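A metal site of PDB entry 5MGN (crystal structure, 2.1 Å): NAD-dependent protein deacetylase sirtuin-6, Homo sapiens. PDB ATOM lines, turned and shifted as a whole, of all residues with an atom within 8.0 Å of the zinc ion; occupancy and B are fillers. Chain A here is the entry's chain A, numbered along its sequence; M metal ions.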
ATOM      1  N   GLU A 134      -3.005 -33.180 -31.946  1.00  0.00           N
ATOM      2  CA  GLU A 134      -2.451 -33.771 -30.679  1.00  0.00           C
ATOM      3  C   GLU A 134      -1.346 -32.851 -30.050  1.00  0.00           C
ATOM      4  O   GLU A 134      -0.518 -32.330 -30.774  1.00  0.00           O
ATOM      5  CB  GLU A 134      -1.877 -35.193 -30.945  1.00  0.00           C
ATOM      6  CG  GLU A 134      -1.045 -35.815 -29.819  1.00  0.00           C
ATOM      7  CD  GLU A 134      -1.054 -37.366 -29.651  1.00  0.00           C
ATOM      8  OE1 GLU A 134      -1.958 -38.113 -30.141  1.00  0.00           O
ATOM      9  OE2 GLU A 134      -0.128 -37.851 -28.904  1.00  0.00           O
ATOM     10  N   CYS A 135      -1.355 -32.679 -28.711  1.00  0.00           N
ATOM     11  CA  CYS A 135      -0.321 -31.854 -28.026  1.00  0.00           C
ATOM     12  C   CYS A 135       0.948 -32.676 -27.952  1.00  0.00           C
ATOM     13  O   CYS A 135       1.000 -33.691 -27.292  1.00  0.00           O
ATOM     14  CB  CYS A 135      -0.650 -31.405 -26.572  1.00  0.00           C
ATOM     15  SG  CYS A 135       0.686 -30.469 -25.622  1.00  0.00           S
ATOM     16  N   ALA A 136       1.969 -32.223 -28.679  1.00  0.00           N
ATOM     17  CA  ALA A 136       3.309 -32.841 -28.623  1.00  0.00           C
ATOM     18  C   ALA A 136       3.922 -32.905 -27.200  1.00  0.00           C
ATOM     19  O   ALA A 136       4.658 -33.822 -26.900  1.00  0.00           O
ATOM     20  CB  ALA A 136       4.196 -32.071 -29.559  1.00  0.00           C
ATOM     21  N   LYS A 137       3.568 -31.965 -26.316  1.00  0.00           N
ATOM     22  CA  LYS A 137       4.001 -32.014 -24.897  1.00  0.00           C
ATOM     23  C   LYS A 137       3.176 -32.948 -24.019  1.00  0.00           C
ATOM     24  O   LYS A 137       3.755 -33.851 -23.436  1.00  0.00           O
ATOM     25  CB  LYS A 137       4.147 -30.573 -24.278  1.00  0.00           C
ATOM     26  CG  LYS A 137       5.024 -29.705 -25.188  1.00  0.00           C
ATOM     27  CD  LYS A 137       5.824 -28.577 -24.546  1.00  0.00           C
ATOM     28  CE  LYS A 137       6.468 -27.751 -25.688  1.00  0.00           C
ATOM     29  NZ  LYS A 137       7.741 -27.095 -25.314  1.00  0.00           N
ATOM     30  N   CYS A 138       1.861 -32.752 -23.902  1.00  0.00           N
ATOM     31  CA  CYS A 138       1.095 -33.567 -22.953  1.00  0.00           C
ATOM     32  C   CYS A 138       0.284 -34.702 -23.567  1.00  0.00           C
ATOM     33  O   CYS A 138      -0.293 -35.456 -22.821  1.00  0.00           O
ATOM     34  CB  CYS A 138       0.220 -32.661 -22.077  1.00  0.00           C
ATOM     35  SG  CYS A 138      -1.267 -31.917 -22.869  1.00  0.00           S
ATOM     36  N   LYS A 139       0.268 -34.827 -24.903  1.00  0.00           N
ATOM     37  CA  LYS A 139      -0.472 -35.888 -25.651  1.00  0.00           C
ATOM     38  C   LYS A 139      -1.974 -35.752 -25.633  1.00  0.00           C
ATOM     39  O   LYS A 139      -2.649 -36.748 -25.962  1.00  0.00           O
ATOM     40  CB  LYS A 139      -0.132 -37.333 -25.177  1.00  0.00           C
ATOM     41  CG  LYS A 139       1.350 -37.665 -25.102  1.00  0.00           C
ATOM     42  CD  LYS A 139       2.100 -37.550 -26.445  1.00  0.00           C
ATOM     43  CE  LYS A 139       3.164 -36.466 -26.366  1.00  0.00           C
ATOM     44  NZ  LYS A 139       4.124 -36.504 -27.511  1.00  0.00           N
ATOM     45  N   THR A 140      -2.509 -34.567 -25.267  1.00  0.00           N
ATOM     46  CA  THR A 140      -3.993 -34.384 -25.264  1.00  0.00           C
ATOM     47  C   THR A 140      -4.441 -34.247 -26.719  1.00  0.00           C
ATOM     48  O   THR A 140      -3.831 -33.548 -27.501  1.00  0.00           O
ATOM     49  CB  THR A 140      -4.517 -33.161 -24.511  1.00  0.00           C
ATOM     50  OG1 THR A 140      -4.238 -33.294 -23.128  1.00  0.00           O
ATOM     51  CG2 THR A 140      -6.069 -33.002 -24.619  1.00  0.00           C
ATOM     52  N   GLN A 141      -5.550 -34.876 -27.048  1.00  0.00           N
ATOM     53  CA  GLN A 141      -6.143 -34.741 -28.394  1.00  0.00           C
ATOM     54  C   GLN A 141      -7.341 -33.798 -28.462  1.00  0.00           C
ATOM     55  O   GLN A 141      -8.070 -33.681 -27.528  1.00  0.00           O
ATOM     56  CB  GLN A 141      -6.434 -36.109 -28.882  1.00  0.00           C
ATOM     57  CG  GLN A 141      -5.152 -36.781 -29.361  1.00  0.00           C
ATOM     58  CD  GLN A 141      -5.322 -38.224 -29.687  1.00  0.00           C
ATOM     59  OE1 GLN A 141      -6.324 -38.852 -29.334  1.00  0.00           O
ATOM     60  NE2 GLN A 141      -4.349 -38.780 -30.411  1.00  0.00           N
ATOM     61  N   TYR A 142      -7.489 -33.065 -29.575  1.00  0.00           N
ATOM     62  CA  TYR A 142      -8.632 -32.120 -29.727  1.00  0.00           C
ATOM     63  C   TYR A 142      -9.348 -32.602 -30.996  1.00  0.00           C
ATOM     64  O   TYR A 142      -8.688 -32.790 -32.031  1.00  0.00           O
ATOM     65  CB  TYR A 142      -8.070 -30.713 -29.933  1.00  0.00           C
ATOM     66  CG  TYR A 142      -7.350 -30.189 -28.682  1.00  0.00           C
ATOM     67  CD1 TYR A 142      -6.006 -30.579 -28.368  1.00  0.00           C
ATOM     68  CD2 TYR A 142      -8.010 -29.335 -27.797  1.00  0.00           C
ATOM     69  CE1 TYR A 142      -5.382 -30.092 -27.216  1.00  0.00           C
ATOM     70  CE2 TYR A 142      -7.393 -28.845 -26.651  1.00  0.00           C
ATOM     71  CZ  TYR A 142      -6.094 -29.233 -26.347  1.00  0.00           C
ATOM     72  OH  TYR A 142      -5.570 -28.730 -25.148  1.00  0.00           O
ATOM     73  N   LEU A 159      -1.960 -23.893 -30.022  1.00  0.00           N
ATOM     74  CA  LEU A 159      -1.397 -24.438 -28.761  1.00  0.00           C
ATOM     75  C   LEU A 159      -2.437 -24.993 -27.811  1.00  0.00           C
ATOM     76  O   LEU A 159      -3.659 -24.659 -27.856  1.00  0.00           O
ATOM     77  CB  LEU A 159      -0.558 -23.398 -27.947  1.00  0.00           C
ATOM     78  CG  LEU A 159       0.595 -22.652 -28.624  1.00  0.00           C
ATOM     79  CD1 LEU A 159       1.244 -21.711 -27.576  1.00  0.00           C
ATOM     80  CD2 LEU A 159       1.630 -23.565 -29.236  1.00  0.00           C
ATOM     81  N   CYS A 160      -1.909 -25.798 -26.935  1.00  0.00           N
ATOM     82  CA  CYS A 160      -2.673 -26.551 -25.992  1.00  0.00           C
ATOM     83  C   CYS A 160      -3.350 -25.647 -24.895  1.00  0.00           C
ATOM     84  O   CYS A 160      -2.731 -24.722 -24.399  1.00  0.00           O
ATOM     85  CB  CYS A 160      -1.697 -27.499 -25.371  1.00  0.00           C
ATOM     86  SG  CYS A 160      -2.457 -28.848 -24.512  1.00  0.00           S
ATOM     87  N   THR A 161      -4.603 -25.952 -24.539  1.00  0.00           N
ATOM     88  CA  THR A 161      -5.343 -25.210 -23.562  1.00  0.00           C
ATOM     89  C   THR A 161      -5.467 -25.917 -22.219  1.00  0.00           C
ATOM     90  O   THR A 161      -6.075 -25.394 -21.331  1.00  0.00           O
ATOM     91  CB  THR A 161      -6.728 -24.757 -24.110  1.00  0.00           C
ATOM     92  OG1 THR A 161      -7.567 -25.872 -24.480  1.00  0.00           O
ATOM     93  CG2 THR A 161      -6.512 -23.956 -25.319  1.00  0.00           C
ATOM     94  N   VAL A 162      -4.827 -27.062 -22.030  1.00  0.00           N
ATOM     95  CA  VAL A 162      -5.065 -27.862 -20.793  1.00  0.00           C
ATOM     96  C   VAL A 162      -4.538 -27.137 -19.537  1.00  0.00           C
ATOM     97  O   VAL A 162      -3.413 -26.572 -19.574  1.00  0.00           O
ATOM     98  CB  VAL A 162      -4.411 -29.285 -20.826  1.00  0.00           C
ATOM     99  CG1 VAL A 162      -4.602 -29.996 -19.486  1.00  0.00           C
ATOM    100  CG2 VAL A 162      -5.013 -30.126 -21.931  1.00  0.00           C
ATOM    101  N   ALA A 163      -5.367 -27.188 -18.462  1.00  0.00           N
ATOM    102  CA  ALA A 163      -5.009 -26.767 -17.100  1.00  0.00           C
ATOM    103  C   ALA A 163      -3.760 -27.459 -16.605  1.00  0.00           C
ATOM    104  O   ALA A 163      -2.975 -26.833 -15.897  1.00  0.00           O
ATOM    105  CB  ALA A 163      -6.165 -27.059 -16.144  1.00  0.00           C
ATOM    106  N   CYS A 171      -0.572 -24.970 -20.437  1.00  0.00           N
ATOM    107  CA  CYS A 171       0.317 -26.001 -21.026  1.00  0.00           C
ATOM    108  C   CYS A 171       1.218 -25.417 -22.122  1.00  0.00           C
ATOM    109  O   CYS A 171       2.445 -25.538 -22.095  1.00  0.00           O
ATOM    110  CB  CYS A 171      -0.492 -27.220 -21.586  1.00  0.00           C
ATOM    111  SG  CYS A 171       0.542 -28.322 -22.638  1.00  0.00           S
ATOM    112  N   ARG A 172       0.570 -24.803 -23.097  1.00  0.00           N
ATOM    113  CA  ARG A 172       1.222 -24.148 -24.249  1.00  0.00           C
ATOM    114  C   ARG A 172       2.008 -25.034 -25.238  1.00  0.00           C
ATOM    115  O   ARG A 172       2.683 -24.498 -26.132  1.00  0.00           O
ATOM    116  CB  ARG A 172       1.999 -22.908 -23.790  1.00  0.00           C
ATOM    117  CG  ARG A 172       1.074 -21.970 -23.020  1.00  0.00           C
ATOM    118  CD  ARG A 172       1.588 -20.548 -22.877  1.00  0.00           C
ATOM    119  NE  ARG A 172       0.887 -19.556 -23.714  1.00  0.00           N
ATOM    120  CZ  ARG A 172       1.354 -19.019 -24.849  1.00  0.00           C
ATOM    121  NH1 ARG A 172       2.536 -19.373 -25.412  1.00  0.00           N
ATOM    122  NH2 ARG A 172       0.614 -18.121 -25.451  1.00  0.00           N
ATOM    123  N   GLY A 173       1.810 -26.353 -25.170  1.00  0.00           N
ATOM    124  CA  GLY A 173       2.554 -27.320 -26.048  1.00  0.00           C
ATOM    125  C   GLY A 173       2.171 -27.145 -27.515  1.00  0.00           C
ATOM    126  O   GLY A 173       1.084 -26.573 -27.821  1.00  0.00           O
ATOM    127  N   GLU A 174       3.035 -27.595 -28.432  1.00  0.00           N
ATOM    128  CA  GLU A 174       2.777 -27.414 -29.884  1.00  0.00           C
ATOM    129  C   GLU A 174       1.690 -28.453 -30.327  1.00  0.00           C
ATOM    130  O   GLU A 174       1.908 -29.694 -30.117  1.00  0.00           O
ATOM    131  CB  GLU A 174       4.075 -27.538 -30.725  1.00  0.00           C
ATOM    132  N   LEU A 175       0.549 -27.966 -30.892  1.00  0.00           N
ATOM    133  CA  LEU A 175      -0.418 -28.902 -31.565  1.00  0.00           C
ATOM    134  C   LEU A 175       0.031 -29.371 -32.945  1.00  0.00           C
ATOM    135  O   LEU A 175       0.459 -28.603 -33.734  1.00  0.00           O
ATOM    136  CB  LEU A 175      -1.838 -28.350 -31.606  1.00  0.00           C
ATOM    137  CG  LEU A 175      -2.482 -27.878 -30.284  1.00  0.00           C
ATOM    138  CD1 LEU A 175      -3.957 -27.590 -30.388  1.00  0.00           C
ATOM    139  CD2 LEU A 175      -2.351 -28.883 -29.153  1.00  0.00           C
HETATM  140 ZN    ZN M   1      -0.571 -30.025 -23.810  1.00  0.00          ZN
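The side-chain sulfur (SG) of Cys 138 sits close to the side-chain hydroxyl (OG1) of Thr 140 (3.3 Å). The backbone NH (N) of Lys 137 sits close to the side-chain sulfur (SG) of Cys 135 (3.3 Å). The backbone NH (N) of Cys 135 is in hydrogen-bond range of the backbone carbonyl oxygen (O) of Thr 140. The backbone NH (N) of Cys 160 is in hydrogen-bond range of the backbone carbonyl oxygen (O) of Gly 173 (3.2 Å). The side-chain sulfur (SG) of Cys 160 lies close to the side-chain hydroxyl (OH) of Tyr 142 (3.2 Å). N of Gly 173 lies close to SG of Cys 171. The backbone carbonyl oxygen of Val 162 is in hydrogen-bond range of the backbone NH of Cys 171.
Of the 19 residues printed, 4 come within 4 Å of the zinc ion.
SG of Cys 138 is bound to the zinc ion (2.2 Å). SG of Cys 135 binds the zinc ion (2.2 Å). SG of Cys 160 binds the zinc ion, 2.3 Å away. SG of Cys 171 is bound to the zinc ion, 2.3 Å away. The zinc ion has four donor atoms within binding distance.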
